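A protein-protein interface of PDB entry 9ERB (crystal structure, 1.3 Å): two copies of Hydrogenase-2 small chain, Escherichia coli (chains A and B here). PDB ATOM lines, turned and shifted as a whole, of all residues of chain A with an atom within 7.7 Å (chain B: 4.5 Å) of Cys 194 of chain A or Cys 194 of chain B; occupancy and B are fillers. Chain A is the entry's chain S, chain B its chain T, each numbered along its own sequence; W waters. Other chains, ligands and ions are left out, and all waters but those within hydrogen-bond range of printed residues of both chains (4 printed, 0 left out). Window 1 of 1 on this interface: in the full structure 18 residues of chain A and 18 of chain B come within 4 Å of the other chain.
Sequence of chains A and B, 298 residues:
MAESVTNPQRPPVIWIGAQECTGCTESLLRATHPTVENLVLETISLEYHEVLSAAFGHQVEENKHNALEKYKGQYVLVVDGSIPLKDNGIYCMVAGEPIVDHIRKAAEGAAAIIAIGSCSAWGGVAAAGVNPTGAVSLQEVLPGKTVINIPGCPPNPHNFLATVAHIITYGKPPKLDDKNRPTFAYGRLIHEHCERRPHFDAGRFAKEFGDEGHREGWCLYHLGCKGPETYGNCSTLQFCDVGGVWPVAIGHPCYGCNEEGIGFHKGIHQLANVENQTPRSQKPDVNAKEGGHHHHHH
Water W3 lies within hydrogen-bond range of the side-chain carboxylate of Glu 192 of chain A (2.6 Å), the backbone carbonyl oxygen of Pro 198 of chain B (2.9 Å) and the guanidinium group of Arg 197 of chain A (2.9 Å). Water W4 lies within hydrogen-bond range of the side-chain carboxylate of Glu 195 of chain B (2.8 Å), the guanidinium group of Arg 196 of chain B (2.9 Å) and a ring nitrogen (NE2) of His 193 of chain A (2.9 Å).
Of the 11 printed residues of chain B, 8 touch a printed residue of chain A. Hydrophobic or aromatic side chains of chain B within 4 Å of the printed part of chain A: His 193 and Pro 198. Hydrophobic or aromatic side chains of chain A that line the printed part of chain B: His 193, Pro 198 and His 199. Among the printed residues, no Asp or Glu carboxylate lies within 4 Å of a Lys or Arg side-chain nitrogen of the other chain.
NE2 of His 199 of chain A lies close to O of Glu 192 of chain B (3.3 Å). A ring nitrogen (NE2) of His 199 of chain A sits at hydrogen-bond distance from a ring nitrogen (ND1) of His 193 of chain B (3.0 Å).
Among the printed residues, merely in contact across the chains: His 191 of chain A with Pro 198 of chain B (3.3 Å), Glu 192 of chain A with Pro 198 of chain B (3.3 Å), His 193 of chain A with Glu 195 of chain B (3.2 Å), His 193 of chain A with Arg 196 of chain B (3.9 Å), His 193 of chain A with Pro 198 of chain B (3.7 Å), Cys 194 of chain A with Cys 194 of chain B (3.8 Å), Cys 194 of chain A with Glu 195 of chain B (3.6 Å), Cys 194 of chain A with Pro 198 of chain B (3.9 Å), Glu 195 of chain A with His 193 of chain B (3.2 Å), Glu 195 of chain A with Cys 194 of chain B (3.6 Å), Glu 195 of chain A with Glu 195 of chain B (3.5 Å), Arg 196 of chain A with His 193 of chain B (3.9 Å), Arg 197 of chain A with Arg 197 of chain B (3.9996 Å), Arg 197 of chain A with Pro 198 of chain B (3.5 Å), Pro 198 of chain A with His 191 of chain B (3.3 Å), Pro 198 of chain A with Glu 192 of chain B (3.2 Å), Pro 198 of chain A with His 193 of chain B (3.6 Å), Pro 198 of chain A with Cys 194 of chain B (3.9 Å) and Pro 198 of chain A with Arg 197 of chain B (3.5 Å).
His 193 of chain A touches Glu 195 of chain B, and with the chains exchanged Glu 195 of chain A touches His 193 of chain B. His 193 of chain A touches Pro 198 of chain B, and with the chains exchanged Pro 198 of chain A touches His 193 of chain B. Cys 194 of chain B touches its own counterpart, Cys 194 of chain A. Glu 195 of chain B touches its own counterpart, Glu 195 of chain A. Positions printed for both chains: 190, 191, 192, 193, 194, 195, 196, 197, 198, 235 and 246.
The guanidinium group (NH1) of Arg 188 of chain A lies within hydrogen-bond range of a ring nitrogen (ND1) of His 193 of chain A, at 3.0 Å. O of His 193 of chain A lies within hydrogen-bond range of OG of Ser 235 of chain A (2.6 Å). The backbone NH (N) of Arg 196 of chain A lies close to the side-chain sulfur (SG) of Cys 194 of chain A (3.4 Å). SG of Cys 194 of chain B lies close to N of Arg 196 of chain B, at 3.4 Å. OE2 of Glu 195 of chain B sits at hydrogen-bond distance from NE1 of Trp 246 of chain B (2.9 Å).
Printed residues of chain B within 4 Å of Glu 192 of chain A: Pro 198 (3.3 Å). Cys 194 of chain A touches just these residues of chain B: Cys 194, Glu 195 and Pro 198. Of the printed residues of chain B, Arg 196 of chain A touches His 193 (3.9 Å). Of the printed residues of chain B, His 199 of chain A touches Glu 192 (3.3 Å) and His 193 (3.0 Å). Of chain A, only Cys 194 (3.8 Å), Glu 195 (3.6 Å) and Pro 198 (3.9 Å) come within 4 Å of Cys 194 of chain B. Of the printed residues of chain A, Pro 198 of chain B touches His 191 (3.3 Å), Glu 192 (3.3 Å), His 193 (3.7 Å), Cys 194 (3.9 Å) and Arg 197 (3.5 Å). The nearest printed residue of chain B that does not touch His 191 of chain A is Glu 195 of chain B (6.3 Å).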
ATOM      1  N   ARG A 188      -6.808   3.631 -13.926  1.00  0.00           N
ATOM      2  CA  ARG A 188      -5.905   4.429 -13.105  1.00  0.00           C
ATOM      3  C   ARG A 188      -4.853   5.089 -13.976  1.00  0.00           C
ATOM      4  O   ARG A 188      -4.421   4.506 -14.976  1.00  0.00           O
ATOM      5  CB  ARG A 188      -5.267   3.490 -12.033  1.00  0.00           C
ATOM      6  CG  ARG A 188      -4.270   4.137 -11.092  1.00  0.00           C
ATOM      7  CD  ARG A 188      -3.891   3.184  -9.969  1.00  0.00           C
ATOM      8  NE  ARG A 188      -5.051   2.943  -9.113  1.00  0.00           N
ATOM      9  CZ  ARG A 188      -5.315   1.813  -8.479  1.00  0.00           C
ATOM     10  NH1 ARG A 188      -4.484   0.781  -8.524  1.00  0.00           N
ATOM     11  NH2 ARG A 188      -6.442   1.717  -7.781  1.00  0.00           N
ATOM     12  N   LEU A 189      -4.427   6.295 -13.582  1.00  0.00           N
ATOM     13  CA  LEU A 189      -3.292   6.942 -14.213  1.00  0.00           C
ATOM     14  C   LEU A 189      -2.028   6.115 -14.010  1.00  0.00           C
ATOM     15  O   LEU A 189      -1.800   5.557 -12.937  1.00  0.00           O
ATOM     16  CB  LEU A 189      -3.052   8.323 -13.605  1.00  0.00           C
ATOM     17  CG  LEU A 189      -4.117   9.372 -13.900  1.00  0.00           C
ATOM     18  CD1 LEU A 189      -3.897  10.588 -13.005  1.00  0.00           C
ATOM     19  CD2 LEU A 189      -4.079   9.768 -15.379  1.00  0.00           C
ATOM     20  N   ILE A 190      -1.168   6.085 -15.022  1.00  0.00           N
ATOM     21  CA  ILE A 190       0.090   5.361 -14.900  1.00  0.00           C
ATOM     22  C   ILE A 190       0.895   5.929 -13.734  1.00  0.00           C
ATOM     23  O   ILE A 190       1.450   5.183 -12.927  1.00  0.00           O
ATOM     24  CB  ILE A 190       0.852   5.407 -16.242  1.00  0.00           C
ATOM     25  CG1 ILE A 190       0.142   4.512 -17.264  1.00  0.00           C
ATOM     26  CG2 ILE A 190       2.282   4.999 -16.055  1.00  0.00           C
ATOM     27  CD1 ILE A 190       0.621   4.662 -18.684  1.00  0.00           C
ATOM     28  N   HIS A 191       0.917   7.255 -13.583  1.00  0.00           N
ATOM     29  CA  HIS A 191       1.675   7.872 -12.487  1.00  0.00           C
ATOM     30  C   HIS A 191       1.111   7.544 -11.116  1.00  0.00           C
ATOM     31  O   HIS A 191       1.853   7.691 -10.135  1.00  0.00           O
ATOM     32  CB  HIS A 191       1.657   9.386 -12.735  1.00  0.00           C
ATOM     33  CG  HIS A 191       2.392  10.243 -11.752  1.00  0.00           C
ATOM     34  ND1 HIS A 191       3.760  10.428 -11.759  1.00  0.00           N
ATOM     35  CD2 HIS A 191       1.897  11.087 -10.808  1.00  0.00           C
ATOM     36  CE1 HIS A 191       4.077  11.304 -10.818  1.00  0.00           C
ATOM     37  NE2 HIS A 191       2.970  11.722 -10.235  1.00  0.00           N
ATOM     38  N   GLU A 192      -0.167   7.156 -11.017  1.00  0.00           N
ATOM     39  CA  GLU A 192      -0.740   6.761  -9.739  1.00  0.00           C
ATOM     40  C   GLU A 192      -0.520   5.277  -9.461  1.00  0.00           C
ATOM     41  O   GLU A 192      -1.070   4.741  -8.483  1.00  0.00           O
ATOM     42  CB  GLU A 192      -2.198   7.166  -9.666  1.00  0.00           C
ATOM     43  CG  GLU A 192      -2.387   8.692  -9.640  1.00  0.00           C
ATOM     44  CD  GLU A 192      -1.669   9.361  -8.494  1.00  0.00           C
ATOM     45  OE1 GLU A 192      -1.849   8.916  -7.350  1.00  0.00           O
ATOM     46  OE2 GLU A 192      -0.837  10.277  -8.712  1.00  0.00           O
ATOM     47  N   HIS A 193       0.318   4.611 -10.261  1.00  0.00           N
ATOM     48  CA  HIS A 193       0.714   3.229  -9.969  1.00  0.00           C
ATOM     49  C   HIS A 193       2.079   2.934 -10.580  1.00  0.00           C
ATOM     50  O   HIS A 193       2.327   1.844 -11.098  1.00  0.00           O
ATOM     51  CB  HIS A 193      -0.354   2.207 -10.386  1.00  0.00           C
ATOM     52  CG  HIS A 193      -0.410   0.995  -9.498  1.00  0.00           C
ATOM     53  ND1 HIS A 193      -1.466   0.743  -8.649  1.00  0.00           N
ATOM     54  CD2 HIS A 193       0.461  -0.030  -9.339  1.00  0.00           C
ATOM     55  CE1 HIS A 193      -1.243  -0.387  -7.999  1.00  0.00           C
ATOM     56  NE2 HIS A 193      -0.072  -0.872  -8.391  1.00  0.00           N
ATOM     57  N   CYS A 194       2.986   3.899 -10.505  1.00  0.00           N
ATOM     58  CA  CYS A 194       4.302   3.800 -11.128  1.00  0.00           C
ATOM     59  C   CYS A 194       5.392   3.592 -10.084  1.00  0.00           C
ATOM     60  O   CYS A 194       5.457   4.323  -9.076  1.00  0.00           O
ATOM     61  CB  CYS A 194       4.615   5.083 -11.912  1.00  0.00           C
ATOM     62  SG  CYS A 194       6.288   5.045 -12.681  1.00  0.00           S
ATOM     63  N   GLU A 195       6.281   2.628 -10.341  1.00  0.00           N
ATOM     64  CA  GLU A 195       7.322   2.281  -9.379  1.00  0.00           C
ATOM     65  C   GLU A 195       8.420   3.327  -9.261  1.00  0.00           C
ATOM     66  O   GLU A 195       9.243   3.218  -8.339  1.00  0.00           O
ATOM     67  CB  GLU A 195       7.939   0.928  -9.720  1.00  0.00           C
ATOM     68  CG  GLU A 195       8.767   0.855 -11.046  1.00  0.00           C
ATOM     69  CD  GLU A 195       7.998   0.685 -12.350  1.00  0.00           C
ATOM     70  OE1 GLU A 195       6.766   0.844 -12.402  1.00  0.00           O
ATOM     71  OE2 GLU A 195       8.701   0.328 -13.340  1.00  0.00           O
ATOM     72  N   ARG A 196       8.433   4.355 -10.124  1.00  0.00           N
ATOM     73  CA  ARG A 196       9.377   5.454  -9.968  1.00  0.00           C
ATOM     74  C   ARG A 196       8.769   6.618  -9.212  1.00  0.00           C
ATOM     75  O   ARG A 196       9.460   7.628  -9.025  1.00  0.00           O
ATOM     76  CB  ARG A 196       9.939   5.897 -11.309  1.00  0.00           C
ATOM     77  CG  ARG A 196      10.602   4.696 -11.996  1.00  0.00           C
ATOM     78  CD  ARG A 196      11.415   5.057 -13.196  1.00  0.00           C
ATOM     79  NE  ARG A 196      12.061   3.872 -13.729  1.00  0.00           N
ATOM     80  CZ  ARG A 196      13.112   3.882 -14.520  1.00  0.00           C
ATOM     81  NH1 ARG A 196      13.643   5.017 -14.923  1.00  0.00           N
ATOM     82  NH2 ARG A 196      13.640   2.734 -14.906  1.00  0.00           N
ATOM     83  N   ARG A 197       7.539   6.485  -8.720  1.00  0.00           N
ATOM     84  CA  ARG A 197       6.959   7.573  -7.932  1.00  0.00           C
ATOM     85  C   ARG A 197       7.843   7.967  -6.755  1.00  0.00           C
ATOM     86  O   ARG A 197       7.885   9.171  -6.437  1.00  0.00           O
ATOM     87  CB  ARG A 197       5.552   7.197  -7.464  1.00  0.00           C
ATOM     88  CG  ARG A 197       4.856   8.283  -6.647  1.00  0.00           C
ATOM     89  CD  ARG A 197       4.655   9.576  -7.420  1.00  0.00           C
ATOM     90  NE  ARG A 197       3.826  10.487  -6.641  1.00  0.00           N
ATOM     91  CZ  ARG A 197       2.504  10.492  -6.651  1.00  0.00           C
ATOM     92  NH1 ARG A 197       1.805   9.806  -7.538  1.00  0.00           N
ATOM     93  NH2 ARG A 197       1.859  11.184  -5.715  1.00  0.00           N
ATOM     94  N   PRO A 198       8.512   7.046  -6.034  1.00  0.00           N
ATOM     95  CA  PRO A 198       9.360   7.507  -4.925  1.00  0.00           C
ATOM     96  C   PRO A 198      10.393   8.521  -5.382  1.00  0.00           C
ATOM     97  O   PRO A 198      10.699   9.474  -4.646  1.00  0.00           O
ATOM     98  CB  PRO A 198      10.056   6.228  -4.458  1.00  0.00           C
ATOM     99  CG  PRO A 198       9.063   5.138  -4.798  1.00  0.00           C
ATOM    100  CD  PRO A 198       8.496   5.573  -6.138  1.00  0.00           C
ATOM    101  N   HIS A 199      10.987   8.301  -6.568  1.00  0.00           N
ATOM    102  CA  HIS A 199      11.977   9.222  -7.118  1.00  0.00           C
ATOM    103  C   HIS A 199      11.353  10.571  -7.452  1.00  0.00           C
ATOM    104  O   HIS A 199      11.919  11.629  -7.113  1.00  0.00           O
ATOM    105  CB  HIS A 199      12.651   8.594  -8.332  1.00  0.00           C
ATOM    106  CG  HIS A 199      13.238   7.260  -8.029  1.00  0.00           C
ATOM    107  ND1 HIS A 199      14.135   7.058  -6.997  1.00  0.00           N
ATOM    108  CD2 HIS A 199      13.000   6.039  -8.566  1.00  0.00           C
ATOM    109  CE1 HIS A 199      14.459   5.780  -6.944  1.00  0.00           C
ATOM    110  NE2 HIS A 199      13.782   5.141  -7.894  1.00  0.00           N
ATOM    111  N   PHE A 200      10.181  10.567  -8.092  1.00  0.00           N
ATOM    112  CA  PHE A 200       9.436  11.802  -8.334  1.00  0.00           C
ATOM    113  C   PHE A 200       9.266  12.557  -7.023  1.00  0.00           C
ATOM    114  O   PHE A 200       9.541  13.765  -6.939  1.00  0.00           O
ATOM    115  CB  PHE A 200       8.077  11.418  -8.940  1.00  0.00           C
ATOM    116  CG  PHE A 200       7.178  12.581  -9.225  1.00  0.00           C
ATOM    117  CD1 PHE A 200       6.298  13.039  -8.267  1.00  0.00           C
ATOM    118  CD2 PHE A 200       7.176  13.196 -10.471  1.00  0.00           C
ATOM    119  CE1 PHE A 200       5.467  14.107  -8.505  1.00  0.00           C
ATOM    120  CE2 PHE A 200       6.329  14.269 -10.741  1.00  0.00           C
ATOM    121  CZ  PHE A 200       5.443  14.715  -9.751  1.00  0.00           C
ATOM    122  N   CYS A 219      13.110   8.885 -11.781  1.00  0.00           N
ATOM    123  CA  CYS A 219      11.881   9.265 -12.466  1.00  0.00           C
ATOM    124  C   CYS A 219      12.203  10.022 -13.750  1.00  0.00           C
ATOM    125  O   CYS A 219      13.198  10.743 -13.833  1.00  0.00           O
ATOM    126  CB  CYS A 219      11.015  10.109 -11.531  1.00  0.00           C
ATOM    127  SG  CYS A 219       9.621  10.975 -12.291  1.00  0.00           S
ATOM    128  N   LEU A 220      11.363   9.804 -14.776  1.00  0.00           N
ATOM    129  CA  LEU A 220      11.518  10.358 -16.117  1.00  0.00           C
ATOM    130  C   LEU A 220      10.632  11.571 -16.400  1.00  0.00           C
ATOM    131  O   LEU A 220      10.503  11.982 -17.570  1.00  0.00           O
ATOM    132  CB  LEU A 220      11.288   9.236 -17.141  1.00  0.00           C
ATOM    133  CG  LEU A 220      12.081   7.963 -16.905  1.00  0.00           C
ATOM    134  CD1 LEU A 220      11.900   6.990 -18.085  1.00  0.00           C
ATOM    135  CD2 LEU A 220      13.546   8.222 -16.743  1.00  0.00           C
ATOM    136  N   CYS A 225       7.846  12.479 -19.378  1.00  0.00           N
ATOM    137  CA  CYS A 225       6.940  11.382 -19.091  1.00  0.00           C
ATOM    138  C   CYS A 225       5.505  11.867 -18.969  1.00  0.00           C
ATOM    139  O   CYS A 225       5.194  12.767 -18.181  1.00  0.00           O
ATOM    140  CB  CYS A 225       7.364  10.684 -17.808  1.00  0.00           C
ATOM    141  SG  CYS A 225       6.407   9.171 -17.481  1.00  0.00           S
ATOM    142  N   GLY A 227       3.015   9.839 -17.946  1.00  0.00           N
ATOM    143  CA  GLY A 227       2.308   9.060 -16.943  1.00  0.00           C
ATOM    144  C   GLY A 227       1.315   9.844 -16.110  1.00  0.00           C
ATOM    145  O   GLY A 227       0.238   9.326 -15.793  1.00  0.00           O
ATOM    146  N   SER A 235       2.459   0.148 -16.291  1.00  0.00           N
ATOM    147  CA  SER A 235       3.435  -0.077 -15.229  1.00  0.00           C
ATOM    148  C   SER A 235       3.205  -1.367 -14.463  1.00  0.00           C
ATOM    149  O   SER A 235       4.147  -1.829 -13.794  1.00  0.00           O
ATOM    150  CB  SER A 235       3.421   1.092 -14.237  1.00  0.00           C
ATOM    151  OG  SER A 235       2.136   1.144 -13.645  1.00  0.00           O
ATOM    152  N   THR A 236       2.020  -1.961 -14.551  1.00  0.00           N
ATOM    153  CA  THR A 236       1.673  -3.153 -13.786  1.00  0.00           C
ATOM    154  C   THR A 236       1.619  -4.359 -14.718  1.00  0.00           C
ATOM    155  O   THR A 236       2.449  -5.265 -14.600  1.00  0.00           O
ATOM    156  CB  THR A 236       0.358  -2.981 -13.024  1.00  0.00           C
ATOM    157  OG1 THR A 236      -0.663  -2.467 -13.893  1.00  0.00           O
ATOM    158  CG2 THR A 236       0.490  -2.036 -11.830  1.00  0.00           C
ATOM    159  N   TRP A 246       8.380  -2.286 -19.804  1.00  0.00           N
ATOM    160  CA  TRP A 246       7.518  -1.232 -20.307  1.00  0.00           C
ATOM    161  C   TRP A 246       8.403  -0.039 -20.588  1.00  0.00           C
ATOM    162  O   TRP A 246       9.580  -0.048 -20.211  1.00  0.00           O
ATOM    163  CB  TRP A 246       6.376  -0.906 -19.338  1.00  0.00           C
ATOM    164  CG  TRP A 246       6.681  -0.203 -18.019  1.00  0.00           C
ATOM    165  CD1 TRP A 246       7.324  -0.728 -16.906  1.00  0.00           C
ATOM    166  CD2 TRP A 246       6.218   1.113 -17.627  1.00  0.00           C
ATOM    167  NE1 TRP A 246       7.288   0.191 -15.873  1.00  0.00           N
ATOM    168  CE2 TRP A 246       6.636   1.324 -16.301  1.00  0.00           C
ATOM    169  CE3 TRP A 246       5.490   2.123 -18.266  1.00  0.00           C
ATOM    170  CZ2 TRP A 246       6.329   2.494 -15.603  1.00  0.00           C
ATOM    171  CZ3 TRP A 246       5.186   3.256 -17.578  1.00  0.00           C
ATOM    172  CH2 TRP A 246       5.600   3.433 -16.257  1.00  0.00           C
ATOM    173  N   VAL A 248       8.977   3.044 -19.542  1.00  0.00           N
ATOM    174  CA  VAL A 248       9.686   3.716 -18.443  1.00  0.00           C
ATOM    175  C   VAL A 248      10.733   2.791 -17.837  1.00  0.00           C
ATOM    176  O   VAL A 248      11.864   3.206 -17.557  1.00  0.00           O
ATOM    177  CB  VAL A 248       8.671   4.220 -17.410  1.00  0.00           C
ATOM    178  CG1 VAL A 248       9.325   4.567 -16.079  1.00  0.00           C
ATOM    179  CG2 VAL A 248       7.938   5.430 -17.977  1.00  0.00           C
ATOM    180  N   ALA A 249      10.392   1.518 -17.641  1.00  0.00           N
ATOM    181  CA  ALA A 249      11.362   0.587 -17.074  1.00  0.00           C
ATOM    182  C   ALA A 249      12.576   0.427 -17.985  1.00  0.00           C
ATOM    183  O   ALA A 249      13.689   0.190 -17.508  1.00  0.00           O
ATOM    184  CB  ALA A 249      10.727  -0.785 -16.829  1.00  0.00           C
ATOM    185  N   ILE B 190      12.908  -1.255  -1.091  1.00  0.00           N
ATOM    186  CA  ILE B 190      11.737  -1.619  -1.893  1.00  0.00           C
ATOM    187  C   ILE B 190      10.756  -0.454  -1.973  1.00  0.00           C
ATOM    188  O   ILE B 190      10.241  -0.145  -3.052  1.00  0.00           O
ATOM    189  CB  ILE B 190      11.098  -2.904  -1.323  1.00  0.00           C
ATOM    190  CG1 ILE B 190      12.041  -4.079  -1.595  1.00  0.00           C
ATOM    191  CG2 ILE B 190       9.687  -3.108  -1.886  1.00  0.00           C
ATOM    192  CD1 ILE B 190      11.631  -5.360  -0.880  1.00  0.00           C
ATOM    193  N   HIS B 191      10.504   0.236  -0.851  1.00  0.00           N
ATOM    194  CA  HIS B 191       9.582   1.373  -0.816  1.00  0.00           C
ATOM    195  C   HIS B 191      10.038   2.548  -1.657  1.00  0.00           C
ATOM    196  O   HIS B 191       9.202   3.399  -2.009  1.00  0.00           O
ATOM    197  CB  HIS B 191       9.428   1.782   0.651  1.00  0.00           C
ATOM    198  CG  HIS B 191       8.494   2.912   0.915  1.00  0.00           C
ATOM    199  ND1 HIS B 191       7.118   2.781   0.938  1.00  0.00           N
ATOM    200  CD2 HIS B 191       8.762   4.188   1.304  1.00  0.00           C
ATOM    201  CE1 HIS B 191       6.587   3.952   1.277  1.00  0.00           C
ATOM    202  NE2 HIS B 191       7.568   4.814   1.493  1.00  0.00           N
ATOM    203  N   GLU B 192      11.337   2.641  -1.949  1.00  0.00           N
ATOM    204  CA  GLU B 192      11.852   3.692  -2.814  1.00  0.00           C
ATOM    205  C   GLU B 192      11.840   3.296  -4.283  1.00  0.00           C
ATOM    206  O   GLU B 192      12.358   4.046  -5.126  1.00  0.00           O
ATOM    207  CB  GLU B 192      13.241   4.125  -2.367  1.00  0.00           C
ATOM    208  CG  GLU B 192      13.223   4.855  -1.003  1.00  0.00           C
ATOM    209  CD  GLU B 192      12.304   6.038  -0.991  1.00  0.00           C
ATOM    210  OE1 GLU B 192      12.430   6.911  -1.888  1.00  0.00           O
ATOM    211  OE2 GLU B 192      11.424   6.145  -0.119  1.00  0.00           O
ATOM    212  N   HIS B 193      11.191   2.180  -4.622  1.00  0.00           N
ATOM    213  CA  HIS B 193      10.950   1.817  -6.031  1.00  0.00           C
ATOM    214  C   HIS B 193       9.735   0.919  -6.132  1.00  0.00           C
ATOM    215  O   HIS B 193       9.709  -0.035  -6.925  1.00  0.00           O
ATOM    216  CB  HIS B 193      12.199   1.185  -6.651  1.00  0.00           C
ATOM    217  CG  HIS B 193      12.349   1.463  -8.107  1.00  0.00           C
ATOM    218  ND1 HIS B 193      13.352   2.264  -8.603  1.00  0.00           N
ATOM    219  CD2 HIS B 193      11.634   1.028  -9.166  1.00  0.00           C
ATOM    220  CE1 HIS B 193      13.226   2.332  -9.921  1.00  0.00           C
ATOM    221  NE2 HIS B 193      12.194   1.589 -10.288  1.00  0.00           N
ATOM    222  N   CYS B 194       8.680   1.254  -5.393  1.00  0.00           N
ATOM    223  CA  CYS B 194       7.446   0.462  -5.306  1.00  0.00           C
ATOM    224  C   CYS B 194       6.311   1.161  -6.049  1.00  0.00           C
ATOM    225  O   CYS B 194       6.048   2.349  -5.834  1.00  0.00           O
ATOM    226  CB  CYS B 194       7.026   0.265  -3.845  1.00  0.00           C
ATOM    227  SG  CYS B 194       5.483  -0.688  -3.715  1.00  0.00           S
ATOM    228  N   GLU B 195       5.631   0.410  -6.920  1.00  0.00           N
ATOM    229  CA  GLU B 195       4.561   0.939  -7.747  1.00  0.00           C
ATOM    230  C   GLU B 195       3.327   1.357  -6.966  1.00  0.00           C
ATOM    231  O   GLU B 195       2.452   2.005  -7.527  1.00  0.00           O
ATOM    232  CB  GLU B 195       4.206  -0.051  -8.850  1.00  0.00           C
ATOM    233  CG  GLU B 195       3.534  -1.340  -8.419  1.00  0.00           C
ATOM    234  CD  GLU B 195       4.416  -2.479  -7.946  1.00  0.00           C
ATOM    235  OE1 GLU B 195       5.601  -2.266  -7.637  1.00  0.00           O
ATOM    236  OE2 GLU B 195       3.872  -3.605  -7.873  1.00  0.00           O
ATOM    237  N   ARG B 196       3.221   1.005  -5.675  1.00  0.00           N
ATOM    238  CA  ARG B 196       2.115   1.466  -4.854  1.00  0.00           C
ATOM    239  C   ARG B 196       2.459   2.716  -4.062  1.00  0.00           C
ATOM    240  O   ARG B 196       1.609   3.195  -3.298  1.00  0.00           O
ATOM    241  CB  ARG B 196       1.655   0.350  -3.922  1.00  0.00           C
ATOM    242  CG  ARG B 196       1.233  -0.883  -4.718  1.00  0.00           C
ATOM    243  CD  ARG B 196       0.409  -1.871  -3.961  1.00  0.00           C
ATOM    244  NE  ARG B 196       0.074  -2.971  -4.855  1.00  0.00           N
ATOM    245  CZ  ARG B 196      -0.891  -3.842  -4.619  1.00  0.00           C
ATOM    246  NH1 ARG B 196      -1.585  -3.835  -3.483  1.00  0.00           N
ATOM    247  NH2 ARG B 196      -1.200  -4.723  -5.560  1.00  0.00           N
ATOM    248  N   ARG B 197       3.647   3.265  -4.249  1.00  0.00           N
ATOM    249  CA  ARG B 197       3.979   4.523  -3.582  1.00  0.00           C
ATOM    250  C   ARG B 197       2.962   5.624  -3.831  1.00  0.00           C
ATOM    251  O   ARG B 197       2.690   6.390  -2.892  1.00  0.00           O
ATOM    252  CB  ARG B 197       5.390   4.941  -3.976  1.00  0.00           C
ATOM    253  CG  ARG B 197       5.829   6.258  -3.338  1.00  0.00           C
ATOM    254  CD  ARG B 197       5.887   6.183  -1.792  1.00  0.00           C
ATOM    255  NE  ARG B 197       6.527   7.386  -1.271  1.00  0.00           N
ATOM    256  CZ  ARG B 197       7.830   7.535  -1.101  1.00  0.00           C
ATOM    257  NH1 ARG B 197       8.670   6.532  -1.239  1.00  0.00           N
ATOM    258  NH2 ARG B 197       8.311   8.758  -0.865  1.00  0.00           N
ATOM    259  N   PRO B 198       2.375   5.784  -5.023  1.00  0.00           N
ATOM    260  CA  PRO B 198       1.354   6.835  -5.161  1.00  0.00           C
ATOM    261  C   PRO B 198       0.233   6.679  -4.162  1.00  0.00           C
ATOM    262  O   PRO B 198      -0.315   7.674  -3.665  1.00  0.00           O
ATOM    263  CB  PRO B 198       0.834   6.623  -6.585  1.00  0.00           C
ATOM    264  CG  PRO B 198       2.039   6.022  -7.324  1.00  0.00           C
ATOM    265  CD  PRO B 198       2.637   5.075  -6.301  1.00  0.00           C
ATOM    266  N   SER B 235      10.253  -5.432  -6.212  1.00  0.00           N
ATOM    267  CA  SER B 235       9.231  -4.720  -6.965  1.00  0.00           C
ATOM    268  C   SER B 235       9.601  -4.528  -8.425  1.00  0.00           C
ATOM    269  O   SER B 235       8.706  -4.273  -9.224  1.00  0.00           O
ATOM    270  CB  SER B 235       8.981  -3.330  -6.357  1.00  0.00           C
ATOM    271  OG  SER B 235      10.199  -2.615  -6.393  1.00  0.00           O
ATOM    272  N   TRP B 246       5.173 -10.466  -7.398  1.00  0.00           N
ATOM    273  CA  TRP B 246       5.898 -10.327  -6.143  1.00  0.00           C
ATOM    274  C   TRP B 246       4.873 -10.211  -5.034  1.00  0.00           C
ATOM    275  O   TRP B 246       3.674 -10.069  -5.307  1.00  0.00           O
ATOM    276  CB  TRP B 246       6.860  -9.147  -6.174  1.00  0.00           C
ATOM    277  CG  TRP B 246       6.322  -7.730  -6.125  1.00  0.00           C
ATOM    278  CD1 TRP B 246       5.679  -7.060  -7.129  1.00  0.00           C
ATOM    279  CD2 TRP B 246       6.575  -6.751  -5.099  1.00  0.00           C
ATOM    280  NE1 TRP B 246       5.454  -5.758  -6.766  1.00  0.00           N
ATOM    281  CE2 TRP B 246       5.997  -5.546  -5.521  1.00  0.00           C
ATOM    282  CE3 TRP B 246       7.189  -6.796  -3.839  1.00  0.00           C
ATOM    283  CZ2 TRP B 246       6.043  -4.383  -4.738  1.00  0.00           C
ATOM    284  CZ3 TRP B 246       7.247  -5.646  -3.079  1.00  0.00           C
ATOM    285  CH2 TRP B 246       6.680  -4.466  -3.525  1.00  0.00           C
HETATM  286  O   HOH W   1      10.991   9.128  -1.834  1.00  0.00           O
HETATM  287  O   HOH W   2      11.335   1.109 -13.052  1.00  0.00           O
HETATM  288  O   HOH W   3      -0.798  10.028  -5.204  1.00  0.00           O
HETATM  289  O   HOH W   4       1.075  -3.425  -7.556  1.00  0.00           O
